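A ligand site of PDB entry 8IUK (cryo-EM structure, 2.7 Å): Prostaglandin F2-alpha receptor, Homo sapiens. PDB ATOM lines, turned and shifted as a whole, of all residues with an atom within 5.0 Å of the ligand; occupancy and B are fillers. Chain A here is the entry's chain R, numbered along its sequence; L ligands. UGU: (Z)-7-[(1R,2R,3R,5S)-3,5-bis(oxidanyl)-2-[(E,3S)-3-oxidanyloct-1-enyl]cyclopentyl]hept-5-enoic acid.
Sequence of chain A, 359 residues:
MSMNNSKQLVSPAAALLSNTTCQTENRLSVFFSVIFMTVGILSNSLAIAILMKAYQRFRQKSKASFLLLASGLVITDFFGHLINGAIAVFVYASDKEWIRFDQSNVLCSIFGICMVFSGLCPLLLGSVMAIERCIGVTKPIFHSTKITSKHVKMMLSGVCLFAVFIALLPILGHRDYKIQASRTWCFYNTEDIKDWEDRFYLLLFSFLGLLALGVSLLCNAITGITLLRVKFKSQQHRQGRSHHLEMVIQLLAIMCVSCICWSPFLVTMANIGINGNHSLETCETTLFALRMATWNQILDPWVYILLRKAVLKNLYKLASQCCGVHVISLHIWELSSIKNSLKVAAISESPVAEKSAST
The side-chain amide oxygen (OE1) of Gln 297 is in hydrogen-bond range of the indole nitrogen (NE1) of Trp 262 (3.0 Å).
The backbone carbonyl oxygen of Ala 293 lies within hydrogen-bond range of the side-chain amide nitrogen of Gln 297, at 2.4 Å.
Ser 29 touches the ligand.
Phe 32 touches the ligand (CB to O2, 3.6 Å).
Phe 36 touches the ligand.
Gly 85 touches the ligand.
Ala 88 touches the ligand (CB to O3, 3.4 Å).
Met 115 touches the ligand (CE to C6, 3.7 Å).
Ser 118 touches the ligand.
CA of Gly 119 touches C20 of the ligand, 3.95 Å away.
OG1 of Thr 184 touches C2 of the ligand (3.8 Å).
Trp 262 touches the ligand (CH2 to C19, 3.8 Å).
Leu 287 touches the ligand.
CD2 of Leu 290 touches C5 of the ligand, 3.5 Å away.
NE2 of Gln 297 touches C17 of the ligand, 3.6 Å away.
18 residues have an atom within 4 Å of the ligand: Ser 29, Phe 32, Ser 33, Phe 36, His 81, Asn 84, Gly 85, Ala 88, Met 115, Ser 118, Gly 119, Thr 184, Trp 262, Leu 287, Leu 290, Arg 291, Thr 294 and Gln 297.
The guanidinium group of Arg 291 lies within salt-bridge range of an oxygen (O1) of the ligand (2.5 Å).
OG of Ser 33 is in hydrogen-bond range of O3 of the ligand, 2.6 Å away.
O4 of the ligand sits at hydrogen-bond distance from OG1 of Thr 294 (2.7 Å).
A ring nitrogen (NE2) of His 81 is in hydrogen-bond range of an oxygen (O5) of the ligand (3.0 Å).
The backbone carbonyl oxygen of Asn 84 is in hydrogen-bond range of an oxygen (O3) of the ligand, 3.1 Å away.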
ATOM      1  N   SER A  29      21.308  25.730 -19.346  1.00  0.00           N
ATOM      2  CA  SER A  29      22.484  24.873 -19.291  1.00  0.00           C
ATOM      3  C   SER A  29      22.087  23.447 -18.924  1.00  0.00           C
ATOM      4  O   SER A  29      22.327  22.507 -19.694  1.00  0.00           O
ATOM      5  CB  SER A  29      23.494  25.406 -18.282  1.00  0.00           C
ATOM      6  OG  SER A  29      23.904  26.724 -18.612  1.00  0.00           O
ATOM      7  N   PHE A  32      20.024  21.964 -21.164  1.00  0.00           N
ATOM      8  CA  PHE A  32      20.580  21.562 -22.420  1.00  0.00           C
ATOM      9  C   PHE A  32      21.177  20.218 -22.238  1.00  0.00           C
ATOM     10  O   PHE A  32      21.587  19.601 -23.196  1.00  0.00           O
ATOM     11  CB  PHE A  32      21.628  22.539 -22.921  1.00  0.00           C
ATOM     12  CG  PHE A  32      21.247  23.237 -24.173  1.00  0.00           C
ATOM     13  CD1 PHE A  32      20.808  22.531 -25.266  1.00  0.00           C
ATOM     14  CD2 PHE A  32      21.349  24.602 -24.259  1.00  0.00           C
ATOM     15  CE1 PHE A  32      20.456  23.176 -26.432  1.00  0.00           C
ATOM     16  CE2 PHE A  32      21.000  25.271 -25.417  1.00  0.00           C
ATOM     17  CZ  PHE A  32      20.555  24.553 -26.509  1.00  0.00           C
ATOM     18  N   SER A  33      21.234  19.738 -21.019  1.00  0.00           N
ATOM     19  CA  SER A  33      21.714  18.372 -20.851  1.00  0.00           C
ATOM     20  C   SER A  33      20.639  17.400 -20.385  1.00  0.00           C
ATOM     21  O   SER A  33      20.783  16.205 -20.599  1.00  0.00           O
ATOM     22  CB  SER A  33      22.911  18.314 -19.922  1.00  0.00           C
ATOM     23  OG  SER A  33      23.711  17.198 -20.230  1.00  0.00           O
ATOM     24  N   PHE A  36      18.262  16.256 -23.529  1.00  0.00           N
ATOM     25  CA  PHE A  36      19.011  15.264 -24.287  1.00  0.00           C
ATOM     26  C   PHE A  36      18.972  13.901 -23.611  1.00  0.00           C
ATOM     27  O   PHE A  36      18.799  12.876 -24.264  1.00  0.00           O
ATOM     28  CB  PHE A  36      20.452  15.728 -24.485  1.00  0.00           C
ATOM     29  CG  PHE A  36      20.585  16.950 -25.345  1.00  0.00           C
ATOM     30  CD1 PHE A  36      19.582  17.314 -26.223  1.00  0.00           C
ATOM     31  CD2 PHE A  36      21.727  17.733 -25.286  1.00  0.00           C
ATOM     32  CE1 PHE A  36      19.709  18.440 -27.021  1.00  0.00           C
ATOM     33  CE2 PHE A  36      21.860  18.858 -26.071  1.00  0.00           C
ATOM     34  CZ  PHE A  36      20.844  19.214 -26.943  1.00  0.00           C
ATOM     35  N   MET A  37      19.124  13.882 -22.280  1.00  0.00           N
ATOM     36  CA  MET A  37      19.094  12.626 -21.549  1.00  0.00           C
ATOM     37  C   MET A  37      17.753  11.928 -21.698  1.00  0.00           C
ATOM     38  O   MET A  37      17.687  10.716 -21.946  1.00  0.00           O
ATOM     39  CB  MET A  37      19.404  12.868 -20.072  1.00  0.00           C
ATOM     40  CG  MET A  37      19.318  11.619 -19.212  1.00  0.00           C
ATOM     41  SD  MET A  37      19.543  11.976 -17.454  1.00  0.00           S
ATOM     42  CE  MET A  37      18.196  13.114 -17.157  1.00  0.00           C
ATOM     43  N   HIS A  81      24.659   7.373 -21.843  1.00  0.00           N
ATOM     44  CA  HIS A  81      23.813   8.559 -21.699  1.00  0.00           C
ATOM     45  C   HIS A  81      23.298   8.685 -20.276  1.00  0.00           C
ATOM     46  O   HIS A  81      23.283   9.779 -19.727  1.00  0.00           O
ATOM     47  CB  HIS A  81      22.628   8.505 -22.661  1.00  0.00           C
ATOM     48  CG  HIS A  81      22.895   9.174 -23.967  1.00  0.00           C
ATOM     49  ND1 HIS A  81      22.905   8.492 -25.167  1.00  0.00           N
ATOM     50  CD2 HIS A  81      23.155  10.466 -24.273  1.00  0.00           C
ATOM     51  CE1 HIS A  81      23.162   9.329 -26.147  1.00  0.00           C
ATOM     52  NE2 HIS A  81      23.321  10.538 -25.638  1.00  0.00           N
ATOM     53  N   ASN A  84      26.167   9.778 -17.990  1.00  0.00           N
ATOM     54  CA  ASN A  84      26.512  11.179 -18.216  1.00  0.00           C
ATOM     55  C   ASN A  84      25.445  12.102 -17.653  1.00  0.00           C
ATOM     56  O   ASN A  84      25.758  13.137 -17.052  1.00  0.00           O
ATOM     57  CB  ASN A  84      26.719  11.437 -19.712  1.00  0.00           C
ATOM     58  CG  ASN A  84      28.013  10.844 -20.230  1.00  0.00           C
ATOM     59  OD1 ASN A  84      29.057  11.486 -20.199  1.00  0.00           O
ATOM     60  ND2 ASN A  84      27.943   9.607 -20.729  1.00  0.00           N
ATOM     61  N   GLY A  85      24.171  11.752 -17.829  1.00  0.00           N
ATOM     62  CA  GLY A  85      23.106  12.578 -17.287  1.00  0.00           C
ATOM     63  C   GLY A  85      23.086  12.594 -15.769  1.00  0.00           C
ATOM     64  O   GLY A  85      22.872  13.645 -15.157  1.00  0.00           O
ATOM     65  N   ALA A  88      25.941  14.789 -14.685  1.00  0.00           N
ATOM     66  CA  ALA A  88      25.636  16.191 -14.935  1.00  0.00           C
ATOM     67  C   ALA A  88      24.642  16.727 -13.903  1.00  0.00           C
ATOM     68  O   ALA A  88      24.794  17.862 -13.433  1.00  0.00           O
ATOM     69  CB  ALA A  88      25.080  16.368 -16.349  1.00  0.00           C
ATOM     70  N   TYR A  92      25.457  19.814 -11.396  1.00  0.00           N
ATOM     71  CA  TYR A  92      24.617  21.012 -11.349  1.00  0.00           C
ATOM     72  C   TYR A  92      23.878  21.155 -10.023  1.00  0.00           C
ATOM     73  O   TYR A  92      23.437  22.261  -9.699  1.00  0.00           O
ATOM     74  CB  TYR A  92      23.615  20.996 -12.501  1.00  0.00           C
ATOM     75  CG  TYR A  92      24.176  21.516 -13.804  1.00  0.00           C
ATOM     76  CD1 TYR A  92      24.842  20.678 -14.689  1.00  0.00           C
ATOM     77  CD2 TYR A  92      24.026  22.850 -14.163  1.00  0.00           C
ATOM     78  CE1 TYR A  92      25.364  21.157 -15.881  1.00  0.00           C
ATOM     79  CE2 TYR A  92      24.532  23.337 -15.346  1.00  0.00           C
ATOM     80  CZ  TYR A  92      25.199  22.479 -16.209  1.00  0.00           C
ATOM     81  OH  TYR A  92      25.704  22.966 -17.392  1.00  0.00           O
ATOM     82  N   PHE A 111      34.175  10.553 -14.885  1.00  0.00           N
ATOM     83  CA  PHE A 111      33.435  11.270 -15.916  1.00  0.00           C
ATOM     84  C   PHE A 111      34.220  11.297 -17.227  1.00  0.00           C
ATOM     85  O   PHE A 111      33.643  11.080 -18.308  1.00  0.00           O
ATOM     86  CB  PHE A 111      33.129  12.692 -15.450  1.00  0.00           C
ATOM     87  CG  PHE A 111      31.979  13.334 -16.169  1.00  0.00           C
ATOM     88  CD1 PHE A 111      31.185  12.607 -17.038  1.00  0.00           C
ATOM     89  CD2 PHE A 111      31.687  14.679 -15.987  1.00  0.00           C
ATOM     90  CE1 PHE A 111      30.132  13.192 -17.703  1.00  0.00           C
ATOM     91  CE2 PHE A 111      30.631  15.275 -16.643  1.00  0.00           C
ATOM     92  CZ  PHE A 111      29.855  14.526 -17.506  1.00  0.00           C
ATOM     93  N   MET A 115      33.147   9.584 -20.722  1.00  0.00           N
ATOM     94  CA  MET A 115      33.068  10.394 -21.927  1.00  0.00           C
ATOM     95  C   MET A 115      33.868   9.776 -23.065  1.00  0.00           C
ATOM     96  O   MET A 115      33.394   9.669 -24.199  1.00  0.00           O
ATOM     97  CB  MET A 115      33.559  11.814 -21.633  1.00  0.00           C
ATOM     98  CG  MET A 115      33.256  12.823 -22.730  1.00  0.00           C
ATOM     99  SD  MET A 115      31.503  13.236 -22.822  1.00  0.00           S
ATOM    100  CE  MET A 115      31.227  13.910 -21.188  1.00  0.00           C
ATOM    101  N   SER A 118      31.929   6.639 -24.278  1.00  0.00           N
ATOM    102  CA  SER A 118      30.774   6.979 -25.092  1.00  0.00           C
ATOM    103  C   SER A 118      31.155   7.694 -26.388  1.00  0.00           C
ATOM    104  O   SER A 118      30.315   7.799 -27.291  1.00  0.00           O
ATOM    105  CB  SER A 118      29.796   7.842 -24.291  1.00  0.00           C
ATOM    106  OG  SER A 118      29.336   7.160 -23.137  1.00  0.00           O
ATOM    107  N   GLY A 119      32.384   8.180 -26.491  1.00  0.00           N
ATOM    108  CA  GLY A 119      32.834   8.782 -27.730  1.00  0.00           C
ATOM    109  C   GLY A 119      33.508   7.822 -28.671  1.00  0.00           C
ATOM    110  O   GLY A 119      33.447   7.990 -29.899  1.00  0.00           O
ATOM    111  N   THR A 184      31.746  21.940 -16.280  1.00  0.00           N
ATOM    112  CA  THR A 184      30.596  21.041 -16.213  1.00  0.00           C
ATOM    113  C   THR A 184      30.874  19.644 -16.736  1.00  0.00           C
ATOM    114  O   THR A 184      30.007  18.769 -16.593  1.00  0.00           O
ATOM    115  CB  THR A 184      29.417  21.627 -17.006  1.00  0.00           C
ATOM    116  OG1 THR A 184      29.585  21.357 -18.409  1.00  0.00           O
ATOM    117  CG2 THR A 184      29.299  23.131 -16.786  1.00  0.00           C
ATOM    118  N   TRP A 185      32.065  19.439 -17.293  1.00  0.00           N
ATOM    119  CA  TRP A 185      32.396  18.120 -17.814  1.00  0.00           C
ATOM    120  C   TRP A 185      33.902  17.991 -17.916  1.00  0.00           C
ATOM    121  O   TRP A 185      34.586  18.916 -18.353  1.00  0.00           O
ATOM    122  CB  TRP A 185      31.740  17.882 -19.179  1.00  0.00           C
ATOM    123  CG  TRP A 185      31.991  18.967 -20.179  1.00  0.00           C
ATOM    124  CD1 TRP A 185      31.348  20.169 -20.258  1.00  0.00           C
ATOM    125  CD2 TRP A 185      32.947  18.947 -21.245  1.00  0.00           C
ATOM    126  NE1 TRP A 185      31.854  20.911 -21.308  1.00  0.00           N
ATOM    127  CE2 TRP A 185      32.841  20.176 -21.927  1.00  0.00           C
ATOM    128  CE3 TRP A 185      33.897  18.016 -21.689  1.00  0.00           C
ATOM    129  CZ2 TRP A 185      33.629  20.493 -23.033  1.00  0.00           C
ATOM    130  CZ3 TRP A 185      34.683  18.337 -22.779  1.00  0.00           C
ATOM    131  CH2 TRP A 185      34.539  19.563 -23.434  1.00  0.00           C
ATOM    132  N   TRP A 262      30.280  14.273 -36.384  1.00  0.00           N
ATOM    133  CA  TRP A 262      31.538  13.916 -35.739  1.00  0.00           C
ATOM    134  C   TRP A 262      32.753  14.602 -36.346  1.00  0.00           C
ATOM    135  O   TRP A 262      33.760  14.758 -35.647  1.00  0.00           O
ATOM    136  CB  TRP A 262      31.728  12.397 -35.775  1.00  0.00           C
ATOM    137  CG  TRP A 262      31.108  11.683 -34.615  1.00  0.00           C
ATOM    138  CD1 TRP A 262      29.889  11.072 -34.584  1.00  0.00           C
ATOM    139  CD2 TRP A 262      31.672  11.515 -33.314  1.00  0.00           C
ATOM    140  NE1 TRP A 262      29.667  10.529 -33.343  1.00  0.00           N
ATOM    141  CE2 TRP A 262      30.742  10.790 -32.540  1.00  0.00           C
ATOM    142  CE3 TRP A 262      32.874  11.912 -32.717  1.00  0.00           C
ATOM    143  CZ2 TRP A 262      30.985  10.451 -31.216  1.00  0.00           C
ATOM    144  CZ3 TRP A 262      33.111  11.567 -31.399  1.00  0.00           C
ATOM    145  CH2 TRP A 262      32.163  10.844 -30.662  1.00  0.00           C
ATOM    146  N   PHE A 265      33.971  18.013 -34.493  1.00  0.00           N
ATOM    147  CA  PHE A 265      34.550  17.780 -33.170  1.00  0.00           C
ATOM    148  C   PHE A 265      35.955  17.211 -33.271  1.00  0.00           C
ATOM    149  O   PHE A 265      36.876  17.659 -32.575  1.00  0.00           O
ATOM    150  CB  PHE A 265      33.641  16.849 -32.366  1.00  0.00           C
ATOM    151  CG  PHE A 265      34.153  16.545 -30.982  1.00  0.00           C
ATOM    152  CD1 PHE A 265      33.974  17.449 -29.953  1.00  0.00           C
ATOM    153  CD2 PHE A 265      34.802  15.342 -30.718  1.00  0.00           C
ATOM    154  CE1 PHE A 265      34.443  17.169 -28.681  1.00  0.00           C
ATOM    155  CE2 PHE A 265      35.270  15.061 -29.446  1.00  0.00           C
ATOM    156  CZ  PHE A 265      35.090  15.979 -28.431  1.00  0.00           C
ATOM    157  N   LEU A 287      31.857  23.158 -27.015  1.00  0.00           N
ATOM    158  CA  LEU A 287      30.537  22.833 -26.470  1.00  0.00           C
ATOM    159  C   LEU A 287      29.533  22.565 -27.590  1.00  0.00           C
ATOM    160  O   LEU A 287      28.730  21.631 -27.504  1.00  0.00           O
ATOM    161  CB  LEU A 287      30.042  23.959 -25.562  1.00  0.00           C
ATOM    162  CG  LEU A 287      28.681  23.756 -24.906  1.00  0.00           C
ATOM    163  CD1 LEU A 287      28.693  22.514 -24.031  1.00  0.00           C
ATOM    164  CD2 LEU A 287      28.281  24.980 -24.104  1.00  0.00           C
ATOM    165  N   LEU A 290      30.291  19.146 -28.974  1.00  0.00           N
ATOM    166  CA  LEU A 290      29.811  18.112 -28.065  1.00  0.00           C
ATOM    167  C   LEU A 290      28.293  17.956 -28.165  1.00  0.00           C
ATOM    168  O   LEU A 290      27.769  16.844 -28.102  1.00  0.00           O
ATOM    169  CB  LEU A 290      30.235  18.430 -26.633  1.00  0.00           C
ATOM    170  CG  LEU A 290      29.824  17.417 -25.560  1.00  0.00           C
ATOM    171  CD1 LEU A 290      30.442  16.057 -25.836  1.00  0.00           C
ATOM    172  CD2 LEU A 290      30.218  17.919 -24.177  1.00  0.00           C
ATOM    173  N   ARG A 291      27.607  19.034 -28.352  1.00  0.00           N
ATOM    174  CA  ARG A 291      26.212  18.900 -28.424  1.00  0.00           C
ATOM    175  C   ARG A 291      25.833  18.281 -29.779  1.00  0.00           C
ATOM    176  O   ARG A 291      25.030  17.359 -29.803  1.00  0.00           O
ATOM    177  CB  ARG A 291      25.601  20.240 -28.113  1.00  0.00           C
ATOM    178  CG  ARG A 291      25.666  20.586 -26.640  1.00  0.00           C
ATOM    179  CD  ARG A 291      25.687  22.089 -26.438  1.00  0.00           C
ATOM    180  NE  ARG A 291      25.626  22.453 -25.038  1.00  0.00           N
ATOM    181  CZ  ARG A 291      24.914  23.459 -24.564  1.00  0.00           C
ATOM    182  NH1 ARG A 291      24.913  23.732 -23.273  1.00  0.00           N
ATOM    183  NH2 ARG A 291      24.195  24.202 -25.385  1.00  0.00           N
ATOM    184  N   ALA A 293      27.510  16.178 -31.087  1.00  0.00           N
ATOM    185  CA  ALA A 293      27.861  14.785 -30.804  1.00  0.00           C
ATOM    186  C   ALA A 293      26.840  14.079 -29.914  1.00  0.00           C
ATOM    187  O   ALA A 293      26.499  12.931 -30.160  1.00  0.00           O
ATOM    188  CB  ALA A 293      29.247  14.703 -30.186  1.00  0.00           C
ATOM    189  N   THR A 294      26.350  14.751 -28.876  1.00  0.00           N
ATOM    190  CA  THR A 294      25.314  14.134 -28.054  1.00  0.00           C
ATOM    191  C   THR A 294      24.170  13.714 -28.955  1.00  0.00           C
ATOM    192  O   THR A 294      23.487  12.724 -28.670  1.00  0.00           O
ATOM    193  CB  THR A 294      24.806  15.076 -26.935  1.00  0.00           C
ATOM    194  OG1 THR A 294      24.160  14.320 -25.906  1.00  0.00           O
ATOM    195  CG2 THR A 294      23.817  16.089 -27.490  1.00  0.00           C
ATOM    196  N   GLN A 297      24.600  10.753 -31.217  1.00  0.00           N
ATOM    197  CA  GLN A 297      24.473   9.584 -30.350  1.00  0.00           C
ATOM    198  C   GLN A 297      23.017   9.290 -30.013  1.00  0.00           C
ATOM    199  O   GLN A 297      22.660   8.124 -29.805  1.00  0.00           O
ATOM    200  CB  GLN A 297      25.287   9.781 -29.070  1.00  0.00           C
ATOM    201  CG  GLN A 297      26.712   9.260 -29.155  1.00  0.00           C
ATOM    202  CD  GLN A 297      27.522   9.954 -30.234  1.00  0.00           C
ATOM    203  OE1 GLN A 297      27.668   9.424 -31.344  1.00  0.00           O
ATOM    204  NE2 GLN A 297      28.055  11.118 -29.915  1.00  0.00           N
HETATM  205  C2  UGU L   1      26.678  20.363 -20.578  1.00  0.00           C
HETATM  206  C3  UGU L   1      26.694  19.002 -21.271  1.00  0.00           C
HETATM  207  C4  UGU L   1      27.419  17.927 -20.466  1.00  0.00           C
HETATM  208  C5  UGU L   1      28.292  17.079 -21.396  1.00  0.00           C
HETATM  209  C6  UGU L   1      28.107  15.792 -21.557  1.00  0.00           C
HETATM  210  C7  UGU L   1      27.000  15.097 -20.775  1.00  0.00           C
HETATM  211  C8  UGU L   1      25.995  14.181 -21.455  1.00  0.00           C
HETATM  212  C9  UGU L   1      24.695  13.935 -20.437  1.00  0.00           C
HETATM  213  O3  UGU L   1      24.668  14.875 -19.409  1.00  0.00           O
HETATM  214  C12 UGU L   1      25.502  14.662 -22.613  1.00  0.00           C
HETATM  215  C11 UGU L   1      24.079  13.929 -22.669  1.00  0.00           C
HETATM  216  O4  UGU L   1      23.238  14.765 -23.388  1.00  0.00           O
HETATM  217  C10 UGU L   1      23.553  13.892 -21.177  1.00  0.00           C
HETATM  218  C13 UGU L   1      26.274  13.943 -23.678  1.00  0.00           C
HETATM  219  C14 UGU L   1      26.414  12.666 -23.470  1.00  0.00           C
HETATM  220  C15 UGU L   1      27.148  11.911 -24.526  1.00  0.00           C
HETATM  221  O5  UGU L   1      26.127  11.697 -25.463  1.00  0.00           O
HETATM  222  C16 UGU L   1      28.215  12.764 -25.205  1.00  0.00           C
HETATM  223  C17 UGU L   1      28.684  12.155 -26.521  1.00  0.00           C
HETATM  224  C18 UGU L   1      30.122  11.648 -26.446  1.00  0.00           C
HETATM  225  C19 UGU L   1      31.044  12.426 -27.388  1.00  0.00           C
HETATM  226  C20 UGU L   1      32.453  12.613 -26.827  1.00  0.00           C
HETATM  227  O1  UGU L   1      26.277  22.548 -21.547  1.00  0.00           O
HETATM  228  C1  UGU L   1      25.855  21.371 -21.386  1.00  0.00           C
HETATM  229  O2  UGU L   1      24.759  21.021 -21.892  1.00  0.00           O
